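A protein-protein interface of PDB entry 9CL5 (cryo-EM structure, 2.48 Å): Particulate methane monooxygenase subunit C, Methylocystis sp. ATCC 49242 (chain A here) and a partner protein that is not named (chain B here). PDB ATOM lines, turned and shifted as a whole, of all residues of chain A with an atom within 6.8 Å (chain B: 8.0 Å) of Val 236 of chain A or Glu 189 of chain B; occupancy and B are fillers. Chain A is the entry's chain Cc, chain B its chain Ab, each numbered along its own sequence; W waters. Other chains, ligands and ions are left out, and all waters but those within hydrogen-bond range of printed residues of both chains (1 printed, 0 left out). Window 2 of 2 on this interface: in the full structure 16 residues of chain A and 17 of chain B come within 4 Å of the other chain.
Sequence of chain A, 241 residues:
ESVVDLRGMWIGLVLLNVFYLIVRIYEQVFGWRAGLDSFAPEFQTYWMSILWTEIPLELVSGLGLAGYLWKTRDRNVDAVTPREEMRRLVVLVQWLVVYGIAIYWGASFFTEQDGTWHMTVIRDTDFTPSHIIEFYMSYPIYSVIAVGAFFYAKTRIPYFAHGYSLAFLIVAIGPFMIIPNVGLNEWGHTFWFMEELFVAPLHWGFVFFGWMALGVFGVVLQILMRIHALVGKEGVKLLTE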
ATOM      1  N   HIS A 228     -21.499   9.230  -6.041  1.00  0.00           N
ATOM      2  CA  HIS A 228     -22.623   9.714  -5.246  1.00  0.00           C
ATOM      3  C   HIS A 228     -22.566  11.225  -5.077  1.00  0.00           C
ATOM      4  O   HIS A 228     -23.503  11.942  -5.450  1.00  0.00           O
ATOM      5  CB  HIS A 228     -22.621   9.012  -3.884  1.00  0.00           C
ATOM      6  CG  HIS A 228     -23.819   9.311  -3.040  1.00  0.00           C
ATOM      7  ND1 HIS A 228     -23.922   8.896  -1.729  1.00  0.00           N
ATOM      8  CD2 HIS A 228     -24.965   9.978  -3.312  1.00  0.00           C
ATOM      9  CE1 HIS A 228     -25.078   9.296  -1.231  1.00  0.00           C
ATOM     10  NE2 HIS A 228     -25.730   9.955  -2.173  1.00  0.00           N
ATOM     11  N   VAL A 231     -23.572  13.107  -8.170  1.00  0.00           N
ATOM     12  CA  VAL A 231     -24.970  13.170  -8.590  1.00  0.00           C
ATOM     13  C   VAL A 231     -25.710  14.271  -7.841  1.00  0.00           C
ATOM     14  O   VAL A 231     -26.561  14.959  -8.417  1.00  0.00           O
ATOM     15  CB  VAL A 231     -25.655  11.803  -8.415  1.00  0.00           C
ATOM     16  CG1 VAL A 231     -26.965  11.777  -9.164  1.00  0.00           C
ATOM     17  CG2 VAL A 231     -24.766  10.697  -8.931  1.00  0.00           C
ATOM     18  N   GLY A 232     -25.405  14.461  -6.561  1.00  0.00           N
ATOM     19  CA  GLY A 232     -26.065  15.480  -5.772  1.00  0.00           C
ATOM     20  C   GLY A 232     -27.386  14.997  -5.210  1.00  0.00           C
ATOM     21  O   GLY A 232     -27.852  13.890  -5.479  1.00  0.00           O
ATOM     22  N   LYS A 233     -28.001  15.862  -4.400  1.00  0.00           N
ATOM     23  CA  LYS A 233     -29.272  15.507  -3.775  1.00  0.00           C
ATOM     24  C   LYS A 233     -30.368  15.305  -4.814  1.00  0.00           C
ATOM     25  O   LYS A 233     -31.016  14.252  -4.841  1.00  0.00           O
ATOM     26  CB  LYS A 233     -29.681  16.585  -2.773  1.00  0.00           C
ATOM     27  CG  LYS A 233     -28.895  16.562  -1.475  1.00  0.00           C
ATOM     28  CD  LYS A 233     -29.740  17.067  -0.317  1.00  0.00           C
ATOM     29  CE  LYS A 233     -29.034  16.864   1.013  1.00  0.00           C
ATOM     30  NZ  LYS A 233     -29.944  17.108   2.165  1.00  0.00           N
ATOM     31  N   GLU A 234     -30.564  16.290  -5.696  1.00  0.00           N
ATOM     32  CA  GLU A 234     -31.633  16.199  -6.685  1.00  0.00           C
ATOM     33  C   GLU A 234     -31.470  14.967  -7.564  1.00  0.00           C
ATOM     34  O   GLU A 234     -32.426  14.207  -7.763  1.00  0.00           O
ATOM     35  CB  GLU A 234     -31.663  17.465  -7.541  1.00  0.00           C
ATOM     36  CG  GLU A 234     -32.849  17.549  -8.486  1.00  0.00           C
ATOM     37  CD  GLU A 234     -32.866  18.839  -9.283  1.00  0.00           C
ATOM     38  OE1 GLU A 234     -31.960  19.675  -9.083  1.00  0.00           O
ATOM     39  OE2 GLU A 234     -33.786  19.017 -10.108  1.00  0.00           O
ATOM     40  N   GLY A 235     -30.258  14.737  -8.070  1.00  0.00           N
ATOM     41  CA  GLY A 235     -30.008  13.531  -8.838  1.00  0.00           C
ATOM     42  C   GLY A 235     -30.273  12.273  -8.036  1.00  0.00           C
ATOM     43  O   GLY A 235     -30.795  11.286  -8.565  1.00  0.00           O
ATOM     44  N   VAL A 236     -29.929  12.292  -6.745  1.00  0.00           N
ATOM     45  CA  VAL A 236     -30.266  11.166  -5.876  1.00  0.00           C
ATOM     46  C   VAL A 236     -31.777  10.979  -5.835  1.00  0.00           C
ATOM     47  O   VAL A 236     -32.281   9.853  -5.924  1.00  0.00           O
ATOM     48  CB  VAL A 236     -29.674  11.376  -4.472  1.00  0.00           C
ATOM     49  CG1 VAL A 236     -30.493  10.639  -3.425  1.00  0.00           C
ATOM     50  CG2 VAL A 236     -28.226  10.912  -4.435  1.00  0.00           C
ATOM     51  N   LYS A 237     -32.520  12.085  -5.738  1.00  0.00           N
ATOM     52  CA  LYS A 237     -33.975  12.010  -5.774  1.00  0.00           C
ATOM     53  C   LYS A 237     -34.453  11.360  -7.065  1.00  0.00           C
ATOM     54  O   LYS A 237     -35.512  10.722  -7.095  1.00  0.00           O
ATOM     55  CB  LYS A 237     -34.566  13.411  -5.611  1.00  0.00           C
ATOM     56  CG  LYS A 237     -36.079  13.485  -5.718  1.00  0.00           C
ATOM     57  CD  LYS A 237     -36.566  14.916  -5.555  1.00  0.00           C
ATOM     58  CE  LYS A 237     -36.032  15.807  -6.664  1.00  0.00           C
ATOM     59  NZ  LYS A 237     -36.601  17.180  -6.594  1.00  0.00           N
ATOM     60  N   LEU A 238     -33.680  11.501  -8.142  1.00  0.00           N
ATOM     61  CA  LEU A 238     -34.008  10.811  -9.384  1.00  0.00           C
ATOM     62  C   LEU A 238     -33.729   9.317  -9.268  1.00  0.00           C
ATOM     63  O   LEU A 238     -34.546   8.486  -9.682  1.00  0.00           O
ATOM     64  CB  LEU A 238     -33.210  11.418 -10.539  1.00  0.00           C
ATOM     65  CG  LEU A 238     -33.382  10.844 -11.948  1.00  0.00           C
ATOM     66  CD1 LEU A 238     -34.830  10.462 -12.232  1.00  0.00           C
ATOM     67  CD2 LEU A 238     -32.862  11.822 -12.988  1.00  0.00           C
ATOM     68  N   LEU A 239     -32.576   8.956  -8.699  1.00  0.00           N
ATOM     69  CA  LEU A 239     -32.143   7.562  -8.737  1.00  0.00           C
ATOM     70  C   LEU A 239     -32.876   6.713  -7.707  1.00  0.00           C
ATOM     71  O   LEU A 239     -33.249   5.569  -7.990  1.00  0.00           O
ATOM     72  CB  LEU A 239     -30.632   7.479  -8.529  1.00  0.00           C
ATOM     73  CG  LEU A 239     -29.778   8.133  -9.619  1.00  0.00           C
ATOM     74  CD1 LEU A 239     -28.297   7.942  -9.337  1.00  0.00           C
ATOM     75  CD2 LEU A 239     -30.142   7.590 -10.993  1.00  0.00           C
ATOM     76  N   THR A 240     -33.090   7.246  -6.506  1.00  0.00           N
ATOM     77  CA  THR A 240     -33.667   6.474  -5.413  1.00  0.00           C
ATOM     78  C   THR A 240     -35.181   6.606  -5.315  1.00  0.00           C
ATOM     79  O   THR A 240     -35.773   6.056  -4.381  1.00  0.00           O
ATOM     80  CB  THR A 240     -33.031   6.888  -4.084  1.00  0.00           C
ATOM     81  OG1 THR A 240     -33.203   8.297  -3.883  1.00  0.00           O
ATOM     82  CG2 THR A 240     -31.551   6.559  -4.083  1.00  0.00           C
ATOM     83  N   GLU A 241     -35.817   7.313  -6.242  1.00  0.00           N
ATOM     84  CA  GLU A 241     -37.270   7.445  -6.229  1.00  0.00           C
ATOM     85  C   GLU A 241     -37.851   7.175  -7.613  1.00  0.00           C
ATOM     86  O   GLU A 241     -38.931   6.596  -7.743  1.00  0.00           O
ATOM     87  CB  GLU A 241     -37.683   8.837  -5.748  1.00  0.00           C
ATOM     88  CG  GLU A 241     -37.292   9.144  -4.311  1.00  0.00           C
ATOM     89  CD  GLU A 241     -37.858  10.464  -3.826  1.00  0.00           C
ATOM     90  OE1 GLU A 241     -38.482  11.179  -4.637  1.00  0.00           O
ATOM     91  OE2 GLU A 241     -37.678  10.786  -2.633  1.00  0.00           O
ATOM     92  N   ILE B 181     -25.469   0.790  -8.269  1.00  0.00           N
ATOM     93  CA  ILE B 181     -25.342   2.201  -7.915  1.00  0.00           C
ATOM     94  C   ILE B 181     -26.551   2.664  -7.112  1.00  0.00           C
ATOM     95  O   ILE B 181     -26.409   3.350  -6.092  1.00  0.00           O
ATOM     96  CB  ILE B 181     -25.139   3.052  -9.182  1.00  0.00           C
ATOM     97  CG1 ILE B 181     -23.729   2.851  -9.741  1.00  0.00           C
ATOM     98  CG2 ILE B 181     -25.396   4.523  -8.890  1.00  0.00           C
ATOM     99  CD1 ILE B 181     -23.494   3.531 -11.069  1.00  0.00           C
ATOM    100  N   THR B 182     -27.757   2.297  -7.555  1.00  0.00           N
ATOM    101  CA  THR B 182     -28.965   2.705  -6.842  1.00  0.00           C
ATOM    102  C   THR B 182     -29.004   2.112  -5.438  1.00  0.00           C
ATOM    103  O   THR B 182     -29.336   2.808  -4.471  1.00  0.00           O
ATOM    104  CB  THR B 182     -30.206   2.289  -7.630  1.00  0.00           C
ATOM    105  OG1 THR B 182     -30.100   2.769  -8.976  1.00  0.00           O
ATOM    106  CG2 THR B 182     -31.457   2.867  -6.994  1.00  0.00           C
ATOM    107  N   SER B 183     -28.665   0.829  -5.308  1.00  0.00           N
ATOM    108  CA  SER B 183     -28.635   0.197  -3.994  1.00  0.00           C
ATOM    109  C   SER B 183     -27.574   0.828  -3.105  1.00  0.00           C
ATOM    110  O   SER B 183     -27.799   1.041  -1.908  1.00  0.00           O
ATOM    111  CB  SER B 183     -28.393  -1.302  -4.138  1.00  0.00           C
ATOM    112  OG  SER B 183     -29.596  -1.981  -4.450  1.00  0.00           O
ATOM    113  N   TYR B 184     -26.405   1.135  -3.675  1.00  0.00           N
ATOM    114  CA  TYR B 184     -25.361   1.797  -2.903  1.00  0.00           C
ATOM    115  C   TYR B 184     -25.829   3.150  -2.387  1.00  0.00           C
ATOM    116  O   TYR B 184     -25.596   3.492  -1.223  1.00  0.00           O
ATOM    117  CB  TYR B 184     -24.098   1.966  -3.748  1.00  0.00           C
ATOM    118  CG  TYR B 184     -23.057   2.817  -3.065  1.00  0.00           C
ATOM    119  CD1 TYR B 184     -22.176   2.260  -2.150  1.00  0.00           C
ATOM    120  CD2 TYR B 184     -22.971   4.181  -3.312  1.00  0.00           C
ATOM    121  CE1 TYR B 184     -21.236   3.033  -1.511  1.00  0.00           C
ATOM    122  CE2 TYR B 184     -22.040   4.960  -2.674  1.00  0.00           C
ATOM    123  CZ  TYR B 184     -21.172   4.381  -1.778  1.00  0.00           C
ATOM    124  OH  TYR B 184     -20.239   5.153  -1.141  1.00  0.00           O
ATOM    125  N   ILE B 185     -26.477   3.941  -3.243  1.00  0.00           N
ATOM    126  CA  ILE B 185     -26.929   5.263  -2.824  1.00  0.00           C
ATOM    127  C   ILE B 185     -28.024   5.145  -1.774  1.00  0.00           C
ATOM    128  O   ILE B 185     -28.064   5.921  -0.812  1.00  0.00           O
ATOM    129  CB  ILE B 185     -27.387   6.082  -4.044  1.00  0.00           C
ATOM    130  CG1 ILE B 185     -26.192   6.407  -4.941  1.00  0.00           C
ATOM    131  CG2 ILE B 185     -28.062   7.368  -3.604  1.00  0.00           C
ATOM    132  CD1 ILE B 185     -26.558   7.144  -6.206  1.00  0.00           C
ATOM    133  N   ARG B 186     -28.926   4.172  -1.932  1.00  0.00           N
ATOM    134  CA  ARG B 186     -29.976   3.975  -0.938  1.00  0.00           C
ATOM    135  C   ARG B 186     -29.394   3.595   0.418  1.00  0.00           C
ATOM    136  O   ARG B 186     -29.813   4.126   1.451  1.00  0.00           O
ATOM    137  CB  ARG B 186     -30.960   2.910  -1.417  1.00  0.00           C
ATOM    138  CG  ARG B 186     -32.136   3.468  -2.191  1.00  0.00           C
ATOM    139  CD  ARG B 186     -33.277   2.475  -2.278  1.00  0.00           C
ATOM    140  NE  ARG B 186     -34.311   2.923  -3.203  1.00  0.00           N
ATOM    141  CZ  ARG B 186     -34.483   2.442  -4.425  1.00  0.00           C
ATOM    142  NH1 ARG B 186     -33.708   1.483  -4.906  1.00  0.00           N
ATOM    143  NH2 ARG B 186     -35.455   2.934  -5.186  1.00  0.00           N
ATOM    144  N   VAL B 187     -28.425   2.679   0.434  1.00  0.00           N
ATOM    145  CA  VAL B 187     -27.814   2.271   1.696  1.00  0.00           C
ATOM    146  C   VAL B 187     -27.011   3.418   2.300  1.00  0.00           C
ATOM    147  O   VAL B 187     -26.973   3.590   3.524  1.00  0.00           O
ATOM    148  CB  VAL B 187     -26.952   1.013   1.485  1.00  0.00           C
ATOM    149  CG1 VAL B 187     -26.166   0.674   2.742  1.00  0.00           C
ATOM    150  CG2 VAL B 187     -27.823  -0.162   1.074  1.00  0.00           C
ATOM    151  N   ALA B 188     -26.367   4.229   1.456  1.00  0.00           N
ATOM    152  CA  ALA B 188     -25.494   5.287   1.955  1.00  0.00           C
ATOM    153  C   ALA B 188     -26.274   6.405   2.632  1.00  0.00           C
ATOM    154  O   ALA B 188     -25.734   7.088   3.510  1.00  0.00           O
ATOM    155  CB  ALA B 188     -24.649   5.851   0.813  1.00  0.00           C
ATOM    156  N   GLU B 189     -27.530   6.614   2.246  1.00  0.00           N
ATOM    157  CA  GLU B 189     -28.357   7.655   2.841  1.00  0.00           C
ATOM    158  C   GLU B 189     -29.211   7.145   3.995  1.00  0.00           C
ATOM    159  O   GLU B 189     -30.157   7.830   4.396  1.00  0.00           O
ATOM    160  CB  GLU B 189     -29.256   8.291   1.779  1.00  0.00           C
ATOM    161  CG  GLU B 189     -28.523   8.742   0.533  1.00  0.00           C
ATOM    162  CD  GLU B 189     -28.781  10.198   0.210  1.00  0.00           C
ATOM    163  OE1 GLU B 189     -29.801  10.491  -0.445  1.00  0.00           O
ATOM    164  OE2 GLU B 189     -27.959  11.050   0.610  1.00  0.00           O
ATOM    165  N   GLY B 190     -28.906   5.969   4.531  1.00  0.00           N
ATOM    166  CA  GLY B 190     -29.678   5.418   5.624  1.00  0.00           C
ATOM    167  C   GLY B 190     -30.960   4.730   5.222  1.00  0.00           C
ATOM    168  O   GLY B 190     -31.741   4.348   6.102  1.00  0.00           O
ATOM    169  N   LYS B 191     -31.209   4.558   3.926  1.00  0.00           N
ATOM    170  CA  LYS B 191     -32.410   3.894   3.427  1.00  0.00           C
ATOM    171  C   LYS B 191     -32.135   2.446   3.039  1.00  0.00           C
ATOM    172  O   LYS B 191     -32.699   1.935   2.068  1.00  0.00           O
ATOM    173  CB  LYS B 191     -32.991   4.664   2.248  1.00  0.00           C
ATOM    174  CG  LYS B 191     -32.856   6.169   2.368  1.00  0.00           C
ATOM    175  CD  LYS B 191     -34.048   6.880   1.755  1.00  0.00           C
ATOM    176  CE  LYS B 191     -34.263   8.242   2.390  1.00  0.00           C
ATOM    177  NZ  LYS B 191     -34.199   8.176   3.876  1.00  0.00           N
ATOM    178  N   ALA B 192     -31.261   1.766   3.786  1.00  0.00           N
ATOM    179  CA  ALA B 192     -30.966   0.367   3.506  1.00  0.00           C
ATOM    180  C   ALA B 192     -32.188  -0.525   3.676  1.00  0.00           C
ATOM    181  O   ALA B 192     -32.235  -1.611   3.086  1.00  0.00           O
ATOM    182  CB  ALA B 192     -29.835  -0.123   4.410  1.00  0.00           C
HETATM  183  O   HOH W   1     -35.740   4.949  -1.215  1.00  0.00           O
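The guanidinium group of Arg 186 of chain B sits at hydrogen-bond distance from the backbone carbonyl oxygen of Thr 240 of chain A (3.2 Å).
The backbone carbonyl oxygen (O) of Val 236 of chain A is in hydrogen-bond range of the side-chain hydroxyl (OG1) of Thr 240 of chain A (2.7 Å).
O of Arg 186 of chain B is in hydrogen-bond range of N of Lys 191 of chain B, at 2.9 Å.
Among the printed residues, merely in contact across the chains: His 228 of chain A with Ile 185 of chain B (3.8 Å), His 228 of chain A with Glu 189 of chain B (3.7 Å), Val 236 of chain A with Ile 185 of chain B (3.6 Å), Val 236 of chain A with Glu 189 of chain B (3.1 Å), Leu 239 of chain A with Thr 182 of chain B (3.4 Å), Leu 239 of chain A with Ile 185 of chain B (3.7 Å) and Thr 240 of chain A with Ile 185 of chain B (3.6 Å).
Of the printed residues of chain B, His 228 of chain A touches Ile 185 (3.8 Å) and Glu 189 (3.7 Å).
No residue of chain B comes within 4 Å of Gly 235 of chain A.
Val 236 of chain A touches two residues of chain B.
Of the printed residues of chain B, Leu 239 of chain A touches Thr 182 and Ile 185.
Of the printed residues of chain B, Thr 240 of chain A touches Ile 185 and Arg 186.
Of the printed residues of chain A, Thr 182 of chain B touches Leu 239 (3.4 Å).
Of the printed residues of chain A, Arg 186 of chain B touches Thr 240.
Glu 189 of chain B touches just these residues of chain A: His 228 and Val 236.
Printed residues of chain A that touch a printed residue of chain B: His 228, Val 236, Leu 239 and Thr 240.
Of the 12 printed residues of chain B, 4 touch a printed residue of chain A.
Among the printed residues, no Asp or Glu carboxylate lies within 4 Å of a Lys or Arg side-chain nitrogen of the other chain.
Water W1 bridges the guanidinium group of Arg 186 of chain B (3.2 Å) and the backbone carbonyl oxygen of Thr 240 of chain A (3.4 Å).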
